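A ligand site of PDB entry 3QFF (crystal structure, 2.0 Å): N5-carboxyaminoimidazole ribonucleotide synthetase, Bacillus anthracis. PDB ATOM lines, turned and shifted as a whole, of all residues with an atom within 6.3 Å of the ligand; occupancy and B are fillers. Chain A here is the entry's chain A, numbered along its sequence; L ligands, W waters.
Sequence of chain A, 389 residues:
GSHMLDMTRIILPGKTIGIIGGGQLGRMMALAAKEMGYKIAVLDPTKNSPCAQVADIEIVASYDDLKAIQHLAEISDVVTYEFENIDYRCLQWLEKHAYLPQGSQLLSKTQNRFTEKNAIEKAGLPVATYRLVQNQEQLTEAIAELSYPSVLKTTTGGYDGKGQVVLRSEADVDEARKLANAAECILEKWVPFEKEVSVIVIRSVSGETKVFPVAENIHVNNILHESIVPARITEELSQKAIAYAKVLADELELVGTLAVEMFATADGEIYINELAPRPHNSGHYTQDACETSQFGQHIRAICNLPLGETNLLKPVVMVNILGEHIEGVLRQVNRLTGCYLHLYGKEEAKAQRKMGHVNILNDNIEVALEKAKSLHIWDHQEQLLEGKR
Tyr 159 touches the ligand. Gln 164 touches the ligand (OE1 to O7, 3.6 Å). CA of Trp 190 touches N4 of the ligand, 3.5 Å away. CE1 of Phe 193 touches N5 of the ligand, at 3.6 Å. OD1 of Asn 222 touches C2 of the ligand (3.5 Å). Phe 263 touches the ligand (CE2 to C4, 3.7 Å). Hydrophobic or aromatic side chains within 4 Å of the ligand: Trp 190, Val 191, Phe 193 and Phe 263. 15 residues have an atom within 4 Å of the ligand: Arg 113, Lys 153, Tyr 159, Asp 160, Gln 164, Glu 188, Lys 189, Trp 190, Val 191, Phe 193, Glu 196, Asn 222, Phe 263, Asn 273 and Glu 274.
N3 of the ligand is in hydrogen-bond range of OE2 of Glu 188 (3.3 Å). The backbone NH of Val 191 lies within hydrogen-bond range of a nitrogen (N4) of the ligand (2.7 Å). OE1 of Glu 274 lies close to O2 of the ligand. The backbone carbonyl oxygen (O) of Lys 189 lies within hydrogen-bond range of a nitrogen (N3) of the ligand, at 2.8 Å. O9 of the ligand sits at hydrogen-bond distance from OE2 of Glu 196 (2.8 Å). The side-chain amino group (NZ) of Lys 153 lies within salt-bridge range of an oxygen (O5) of the ligand (2.8 Å). The side-chain amide nitrogen (ND2) of Asn 273 lies within hydrogen-bond range of an oxygen (O4) of the ligand (2.9 Å). The guanidinium group (NH1) of Arg 113 is in salt-bridge range of an oxygen (O2) of the ligand (2.7 Å). An oxygen (O1) of the ligand lies close to the backbone carbonyl oxygen (O) of Asp 160, at 3.0 Å.
The backbone carbonyl oxygen (O) of Glu 274 lies within hydrogen-bond range of the backbone NH (N) of Glu 261 (2.9 Å). NH2 of Arg 113 is in salt-bridge range of OE1 of Glu 274. The side-chain carboxylate (OE1) of Glu 196 lies within hydrogen-bond range of a ring nitrogen (ND1) of His 219 (3.0 Å). The side-chain amino group (NZ) of Lys 153 lies within salt-bridge range of the side-chain carboxylate (OE1) of Glu 188 (3.0 Å). The backbone NH (N) of Asn 273 is in hydrogen-bond range of the backbone carbonyl oxygen (O) of Glu 261 (2.8 Å). The backbone carbonyl oxygen of Asp 160 lies within hydrogen-bond range of the side-chain amide nitrogen of Asn 222, at 2.9 Å. N of Glu 188 is in hydrogen-bond range of O of Val 151 (2.9 Å).
Water W1 lies within hydrogen-bond range of the side-chain carboxylate of Glu 274 (2.4 Å), an oxygen (O3) of the ligand (2.6 Å) and the side-chain carboxylate of Glu 261 (3.1 Å).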
ATOM      1  N   ARG A 113       6.242   0.374 -14.042  1.00  0.00           N
ATOM      2  CA  ARG A 113       7.347   0.304 -15.032  1.00  0.00           C
ATOM      3  C   ARG A 113       7.952   1.655 -15.336  1.00  0.00           C
ATOM      4  O   ARG A 113       9.162   1.783 -15.532  1.00  0.00           O
ATOM      5  CB  ARG A 113       6.876  -0.321 -16.350  1.00  0.00           C
ATOM      6  CG  ARG A 113       6.466  -1.785 -16.246  1.00  0.00           C
ATOM      7  CD  ARG A 113       6.376  -2.398 -17.651  1.00  0.00           C
ATOM      8  NE  ARG A 113       5.776  -3.734 -17.610  1.00  0.00           N
ATOM      9  CZ  ARG A 113       6.477  -4.858 -17.461  1.00  0.00           C
ATOM     10  NH1 ARG A 113       5.837  -6.022 -17.424  1.00  0.00           N
ATOM     11  NH2 ARG A 113       7.800  -4.816 -17.337  1.00  0.00           N
ATOM     12  N   ALA A 128      16.653   0.936 -21.852  1.00  0.00           N
ATOM     13  CA  ALA A 128      16.181   1.198 -23.213  1.00  0.00           C
ATOM     14  C   ALA A 128      15.394   2.498 -23.197  1.00  0.00           C
ATOM     15  O   ALA A 128      14.705   2.811 -22.219  1.00  0.00           O
ATOM     16  CB  ALA A 128      15.316   0.071 -23.701  1.00  0.00           C
ATOM     17  N   VAL A 151       8.194  -1.961 -28.140  1.00  0.00           N
ATOM     18  CA  VAL A 151       7.330  -2.767 -27.300  1.00  0.00           C
ATOM     19  C   VAL A 151       6.475  -1.857 -26.410  1.00  0.00           C
ATOM     20  O   VAL A 151       6.992  -0.998 -25.698  1.00  0.00           O
ATOM     21  CB  VAL A 151       8.139  -3.739 -26.414  1.00  0.00           C
ATOM     22  CG1 VAL A 151       7.228  -4.698 -25.698  1.00  0.00           C
ATOM     23  CG2 VAL A 151       9.177  -4.498 -27.247  1.00  0.00           C
ATOM     24  N   LYS A 153       4.157  -1.875 -23.219  1.00  0.00           N
ATOM     25  CA  LYS A 153       3.819  -2.670 -22.036  1.00  0.00           C
ATOM     26  C   LYS A 153       2.982  -1.821 -21.085  1.00  0.00           C
ATOM     27  O   LYS A 153       3.149  -0.608 -21.047  1.00  0.00           O
ATOM     28  CB  LYS A 153       5.083  -3.136 -21.308  1.00  0.00           C
ATOM     29  CG  LYS A 153       6.274  -3.429 -22.193  1.00  0.00           C
ATOM     30  CD  LYS A 153       7.409  -4.080 -21.400  1.00  0.00           C
ATOM     31  CE  LYS A 153       8.718  -3.969 -22.159  1.00  0.00           C
ATOM     32  NZ  LYS A 153       9.913  -4.119 -21.261  1.00  0.00           N
ATOM     33  N   GLY A 158       1.406  -6.819 -14.076  1.00  0.00           N
ATOM     34  CA  GLY A 158       1.820  -7.790 -15.090  1.00  0.00           C
ATOM     35  C   GLY A 158       1.090  -9.115 -14.899  1.00  0.00           C
ATOM     36  O   GLY A 158      -0.141  -9.140 -14.769  1.00  0.00           O
ATOM     37  N   TYR A 159       1.821 -10.230 -14.905  1.00  0.00           N
ATOM     38  CA  TYR A 159       3.255 -10.274 -15.171  1.00  0.00           C
ATOM     39  C   TYR A 159       3.360 -11.215 -16.367  1.00  0.00           C
ATOM     40  O   TYR A 159       3.999 -12.276 -16.304  1.00  0.00           O
ATOM     41  CB  TYR A 159       3.993 -10.814 -13.939  1.00  0.00           C
ATOM     42  CG  TYR A 159       3.290 -10.511 -12.626  1.00  0.00           C
ATOM     43  CD1 TYR A 159       2.342 -11.402 -12.100  1.00  0.00           C
ATOM     44  CD2 TYR A 159       3.558  -9.331 -11.934  1.00  0.00           C
ATOM     45  CE1 TYR A 159       1.689 -11.129 -10.898  1.00  0.00           C
ATOM     46  CE2 TYR A 159       2.896  -9.046 -10.730  1.00  0.00           C
ATOM     47  CZ  TYR A 159       1.977  -9.942 -10.218  1.00  0.00           C
ATOM     48  OH  TYR A 159       1.321  -9.665  -9.036  1.00  0.00           O
ATOM     49  N   ASP A 160       2.735 -10.784 -17.454  1.00  0.00           N
ATOM     50  CA  ASP A 160       2.175 -11.688 -18.460  1.00  0.00           C
ATOM     51  C   ASP A 160       2.792 -11.524 -19.857  1.00  0.00           C
ATOM     52  O   ASP A 160       3.837 -10.884 -20.020  1.00  0.00           O
ATOM     53  CB  ASP A 160       0.659 -11.428 -18.543  1.00  0.00           C
ATOM     54  CG  ASP A 160      -0.155 -12.704 -18.559  1.00  0.00           C
ATOM     55  OD1 ASP A 160      -1.301 -12.680 -18.068  1.00  0.00           O
ATOM     56  OD2 ASP A 160       0.345 -13.745 -19.045  1.00  0.00           O
ATOM     57  N   GLY A 161       2.129 -12.122 -20.844  1.00  0.00           N
ATOM     58  CA  GLY A 161       2.397 -11.886 -22.249  1.00  0.00           C
ATOM     59  C   GLY A 161       1.293 -11.014 -22.846  1.00  0.00           C
ATOM     60  O   GLY A 161       1.505 -10.352 -23.867  1.00  0.00           O
ATOM     61  N   GLN A 164       1.378  -6.834 -22.968  1.00  0.00           N
ATOM     62  CA  GLN A 164       2.266  -6.173 -23.942  1.00  0.00           C
ATOM     63  C   GLN A 164       1.977  -6.482 -25.416  1.00  0.00           C
ATOM     64  O   GLN A 164       1.344  -7.488 -25.746  1.00  0.00           O
ATOM     65  CB  GLN A 164       3.753  -6.372 -23.583  1.00  0.00           C
ATOM     66  CG  GLN A 164       4.335  -7.758 -23.757  1.00  0.00           C
ATOM     67  CD  GLN A 164       5.836  -7.767 -23.478  1.00  0.00           C
ATOM     68  OE1 GLN A 164       6.275  -7.475 -22.360  1.00  0.00           O
ATOM     69  NE2 GLN A 164       6.631  -8.088 -24.501  1.00  0.00           N
ATOM     70  N   GLU A 188       8.842   1.162 -25.255  1.00  0.00           N
ATOM     71  CA  GLU A 188      10.303   1.059 -25.197  1.00  0.00           C
ATOM     72  C   GLU A 188      10.889   0.723 -26.560  1.00  0.00           C
ATOM     73  O   GLU A 188      10.315  -0.080 -27.309  1.00  0.00           O
ATOM     74  CB  GLU A 188      10.725  -0.045 -24.249  1.00  0.00           C
ATOM     75  CG  GLU A 188      10.281   0.111 -22.803  1.00  0.00           C
ATOM     76  CD  GLU A 188      10.751  -1.056 -21.941  1.00  0.00           C
ATOM     77  OE1 GLU A 188      10.228  -1.211 -20.828  1.00  0.00           O
ATOM     78  OE2 GLU A 188      11.623  -1.837 -22.400  1.00  0.00           O
ATOM     79  N   LYS A 189      12.047   1.314 -26.875  1.00  0.00           N
ATOM     80  CA  LYS A 189      12.834   0.895 -28.031  1.00  0.00           C
ATOM     81  C   LYS A 189      13.210  -0.569 -27.904  1.00  0.00           C
ATOM     82  O   LYS A 189      13.566  -1.046 -26.829  1.00  0.00           O
ATOM     83  CB  LYS A 189      14.113   1.723 -28.179  1.00  0.00           C
ATOM     84  CG  LYS A 189      14.112   2.707 -29.326  1.00  0.00           C
ATOM     85  CD  LYS A 189      15.429   3.458 -29.398  1.00  0.00           C
ATOM     86  CE  LYS A 189      15.290   4.772 -30.162  1.00  0.00           C
ATOM     87  NZ  LYS A 189      16.094   5.859 -29.549  1.00  0.00           N
ATOM     88  N   TRP A 190      13.102  -1.289 -29.015  1.00  0.00           N
ATOM     89  CA  TRP A 190      13.534  -2.675 -29.088  1.00  0.00           C
ATOM     90  C   TRP A 190      15.043  -2.738 -28.899  1.00  0.00           C
ATOM     91  O   TRP A 190      15.801  -2.058 -29.590  1.00  0.00           O
ATOM     92  CB  TRP A 190      13.155  -3.285 -30.437  1.00  0.00           C
ATOM     93  CG  TRP A 190      13.532  -4.720 -30.611  1.00  0.00           C
ATOM     94  CD1 TRP A 190      14.663  -5.222 -31.220  1.00  0.00           C
ATOM     95  CD2 TRP A 190      12.781  -5.858 -30.181  1.00  0.00           C
ATOM     96  NE1 TRP A 190      14.650  -6.598 -31.186  1.00  0.00           N
ATOM     97  CE2 TRP A 190      13.510  -7.019 -30.558  1.00  0.00           C
ATOM     98  CE3 TRP A 190      11.553  -6.019 -29.509  1.00  0.00           C
ATOM     99  CZ2 TRP A 190      13.056  -8.317 -30.276  1.00  0.00           C
ATOM    100  CZ3 TRP A 190      11.109  -7.308 -29.238  1.00  0.00           C
ATOM    101  CH2 TRP A 190      11.853  -8.440 -29.623  1.00  0.00           C
ATOM    102  N   VAL A 191      15.473  -3.547 -27.936  1.00  0.00           N
ATOM    103  CA  VAL A 191      16.892  -3.742 -27.690  1.00  0.00           C
ATOM    104  C   VAL A 191      17.323  -5.012 -28.409  1.00  0.00           C
ATOM    105  O   VAL A 191      16.778  -6.086 -28.129  1.00  0.00           O
ATOM    106  CB  VAL A 191      17.230  -3.847 -26.182  1.00  0.00           C
ATOM    107  CG1 VAL A 191      18.731  -3.821 -25.950  1.00  0.00           C
ATOM    108  CG2 VAL A 191      16.554  -2.728 -25.390  1.00  0.00           C
ATOM    109  N   PRO A 192      18.252  -4.894 -29.374  1.00  0.00           N
ATOM    110  CA  PRO A 192      18.801  -6.082 -30.026  1.00  0.00           C
ATOM    111  C   PRO A 192      19.831  -6.734 -29.108  1.00  0.00           C
ATOM    112  O   PRO A 192      21.010  -6.371 -29.129  1.00  0.00           O
ATOM    113  CB  PRO A 192      19.474  -5.513 -31.289  1.00  0.00           C
ATOM    114  CG  PRO A 192      19.136  -4.034 -31.327  1.00  0.00           C
ATOM    115  CD  PRO A 192      18.831  -3.658 -29.912  1.00  0.00           C
ATOM    116  N   PHE A 193      19.401  -7.652 -28.255  1.00  0.00           N
ATOM    117  CA  PHE A 193      20.313  -8.253 -27.296  1.00  0.00           C
ATOM    118  C   PHE A 193      20.670  -9.672 -27.699  1.00  0.00           C
ATOM    119  O   PHE A 193      19.903 -10.338 -28.396  1.00  0.00           O
ATOM    120  CB  PHE A 193      19.729  -8.221 -25.868  1.00  0.00           C
ATOM    121  CG  PHE A 193      18.479  -9.014 -25.709  1.00  0.00           C
ATOM    122  CD1 PHE A 193      17.229  -8.405 -25.833  1.00  0.00           C
ATOM    123  CD2 PHE A 193      18.534 -10.386 -25.429  1.00  0.00           C
ATOM    124  CE1 PHE A 193      16.058  -9.151 -25.688  1.00  0.00           C
ATOM    125  CE2 PHE A 193      17.371 -11.134 -25.295  1.00  0.00           C
ATOM    126  CZ  PHE A 193      16.124 -10.515 -25.418  1.00  0.00           C
ATOM    127  N   GLU A 196      19.672 -12.590 -22.199  1.00  0.00           N
ATOM    128  CA  GLU A 196      19.052 -12.048 -20.978  1.00  0.00           C
ATOM    129  C   GLU A 196      19.790 -12.538 -19.740  1.00  0.00           C
ATOM    130  O   GLU A 196      20.025 -13.740 -19.583  1.00  0.00           O
ATOM    131  CB  GLU A 196      17.586 -12.411 -20.881  1.00  0.00           C
ATOM    132  CG  GLU A 196      16.700 -11.577 -21.763  1.00  0.00           C
ATOM    133  CD  GLU A 196      15.250 -11.826 -21.501  1.00  0.00           C
ATOM    134  OE1 GLU A 196      14.722 -12.848 -21.999  1.00  0.00           O
ATOM    135  OE2 GLU A 196      14.628 -10.997 -20.803  1.00  0.00           O
ATOM    136  N   HIS A 219      13.865 -17.397 -21.399  1.00  0.00           N
ATOM    137  CA  HIS A 219      12.412 -17.282 -21.285  1.00  0.00           C
ATOM    138  C   HIS A 219      11.709 -17.922 -22.484  1.00  0.00           C
ATOM    139  O   HIS A 219      12.229 -17.889 -23.601  1.00  0.00           O
ATOM    140  CB  HIS A 219      11.973 -15.821 -21.140  1.00  0.00           C
ATOM    141  CG  HIS A 219      12.470 -15.164 -19.892  1.00  0.00           C
ATOM    142  ND1 HIS A 219      13.715 -14.588 -19.814  1.00  0.00           N
ATOM    143  CD2 HIS A 219      11.915 -15.036 -18.670  1.00  0.00           C
ATOM    144  CE1 HIS A 219      13.895 -14.108 -18.599  1.00  0.00           C
ATOM    145  NE2 HIS A 219      12.820 -14.367 -17.878  1.00  0.00           N
ATOM    146  N   ASN A 222       7.061 -15.862 -22.288  1.00  0.00           N
ATOM    147  CA  ASN A 222       7.214 -14.904 -21.184  1.00  0.00           C
ATOM    148  C   ASN A 222       7.233 -15.518 -19.780  1.00  0.00           C
ATOM    149  O   ASN A 222       6.842 -14.888 -18.790  1.00  0.00           O
ATOM    150  CB  ASN A 222       6.181 -13.778 -21.281  1.00  0.00           C
ATOM    151  CG  ASN A 222       6.734 -12.540 -21.998  1.00  0.00           C
ATOM    152  OD1 ASN A 222       7.667 -12.634 -22.797  1.00  0.00           O
ATOM    153  ND2 ASN A 222       6.148 -11.382 -21.691  1.00  0.00           N
ATOM    154  N   GLU A 261      17.059  -7.679 -13.517  1.00  0.00           N
ATOM    155  CA  GLU A 261      17.049  -8.329 -14.825  1.00  0.00           C
ATOM    156  C   GLU A 261      17.541  -7.363 -15.873  1.00  0.00           C
ATOM    157  O   GLU A 261      17.182  -6.193 -15.856  1.00  0.00           O
ATOM    158  CB  GLU A 261      15.666  -8.869 -15.186  1.00  0.00           C
ATOM    159  CG  GLU A 261      15.229 -10.027 -14.280  1.00  0.00           C
ATOM    160  CD  GLU A 261      13.950 -10.679 -14.770  1.00  0.00           C
ATOM    161  OE1 GLU A 261      12.854 -10.226 -14.353  1.00  0.00           O
ATOM    162  OE2 GLU A 261      14.029 -11.609 -15.595  1.00  0.00           O
ATOM    163  N   PHE A 263      19.356  -6.890 -20.133  1.00  0.00           N
ATOM    164  CA  PHE A 263      19.657  -7.322 -21.494  1.00  0.00           C
ATOM    165  C   PHE A 263      21.138  -7.033 -21.805  1.00  0.00           C
ATOM    166  O   PHE A 263      21.635  -5.907 -21.576  1.00  0.00           O
ATOM    167  CB  PHE A 263      18.803  -6.571 -22.533  1.00  0.00           C
ATOM    168  CG  PHE A 263      17.307  -6.653 -22.315  1.00  0.00           C
ATOM    169  CD1 PHE A 263      16.559  -5.483 -22.209  1.00  0.00           C
ATOM    170  CD2 PHE A 263      16.639  -7.875 -22.251  1.00  0.00           C
ATOM    171  CE1 PHE A 263      15.179  -5.522 -22.031  1.00  0.00           C
ATOM    172  CE2 PHE A 263      15.257  -7.925 -22.065  1.00  0.00           C
ATOM    173  CZ  PHE A 263      14.523  -6.749 -21.949  1.00  0.00           C
ATOM    174  N   ASN A 273      16.335  -4.090 -17.419  1.00  0.00           N
ATOM    175  CA  ASN A 273      14.955  -4.347 -17.857  1.00  0.00           C
ATOM    176  C   ASN A 273      13.945  -4.105 -16.727  1.00  0.00           C
ATOM    177  O   ASN A 273      13.064  -3.244 -16.845  1.00  0.00           O
ATOM    178  CB  ASN A 273      14.825  -5.785 -18.395  1.00  0.00           C
ATOM    179  CG  ASN A 273      13.397  -6.147 -18.810  1.00  0.00           C
ATOM    180  OD1 ASN A 273      12.728  -5.424 -19.540  1.00  0.00           O
ATOM    181  ND2 ASN A 273      12.947  -7.328 -18.372  1.00  0.00           N
ATOM    182  N   GLU A 274      14.061  -4.871 -15.648  1.00  0.00           N
ATOM    183  CA  GLU A 274      13.171  -4.718 -14.492  1.00  0.00           C
ATOM    184  C   GLU A 274      13.809  -5.142 -13.183  1.00  0.00           C
ATOM    185  O   GLU A 274      14.844  -5.819 -13.172  1.00  0.00           O
ATOM    186  CB  GLU A 274      11.821  -5.412 -14.714  1.00  0.00           C
ATOM    187  CG  GLU A 274      11.869  -6.906 -14.956  1.00  0.00           C
ATOM    188  CD  GLU A 274      10.497  -7.473 -15.282  1.00  0.00           C
ATOM    189  OE1 GLU A 274       9.600  -6.679 -15.630  1.00  0.00           O
ATOM    190  OE2 GLU A 274      10.309  -8.696 -15.176  1.00  0.00           O
HETATM  191  P1  LIG L   1       7.413  -9.208 -17.863  1.00  0.00           P
HETATM  192  O1  LIG L   1       6.078  -9.772 -18.294  1.00  0.00           O
HETATM  193  O2  LIG L   1       7.299  -8.207 -16.740  1.00  0.00           O
HETATM  194  O3  LIG L   1       8.465 -10.266 -17.658  1.00  0.00           O
HETATM  195  P2  LIG L   1       9.394  -7.884 -19.540  1.00  0.00           P
HETATM  196  O4  LIG L   1      10.416  -8.657 -18.728  1.00  0.00           O
HETATM  197  O5  LIG L   1       9.461  -6.375 -19.585  1.00  0.00           O
HETATM  198  O6  LIG L   1       7.886  -8.329 -19.143  1.00  0.00           O
HETATM  199  O7  LIG L   1       9.505  -8.373 -21.067  1.00  0.00           O
HETATM  200  C1  LIG L   1       9.176  -9.718 -21.406  1.00  0.00           C
HETATM  201  C2  LIG L   1      10.102 -10.201 -22.515  1.00  0.00           C
HETATM  202  O8  LIG L   1       9.964  -9.343 -23.651  1.00  0.00           O
HETATM  203  C3  LIG L   1      11.561 -10.153 -22.103  1.00  0.00           C
HETATM  204  O9  LIG L   1      12.006 -11.420 -21.625  1.00  0.00           O
HETATM  205  C4  LIG L   1      12.289  -9.729 -23.359  1.00  0.00           C
HETATM  206  O10 LIG L   1      12.767 -10.877 -24.059  1.00  0.00           O
HETATM  207  C5  LIG L   1      11.238  -9.028 -24.207  1.00  0.00           C
HETATM  208  N1  LIG L   1      11.461  -7.557 -24.195  1.00  0.00           N
HETATM  209  C6  LIG L   1      10.902  -6.685 -23.337  1.00  0.00           C
HETATM  210  N2  LIG L   1      11.304  -5.409 -23.595  1.00  0.00           N
HETATM  211  C7  LIG L   1      12.137  -5.457 -24.649  1.00  0.00           C
HETATM  212  C8  LIG L   1      12.918  -4.475 -25.437  1.00  0.00           C
HETATM  213  N3  LIG L   1      12.889  -3.144 -25.137  1.00  0.00           N
HETATM  214  N4  LIG L   1      13.665  -4.939 -26.461  1.00  0.00           N
HETATM  215  C9  LIG L   1      13.716  -6.253 -26.772  1.00  0.00           C
HETATM  216  N5  LIG L   1      13.026  -7.201 -26.103  1.00  0.00           N
HETATM  217  C10 LIG L   1      12.237  -6.875 -25.050  1.00  0.00           C
HETATM  218  O   HOH W   1      10.907 -10.408 -16.762  1.00  0.00           O
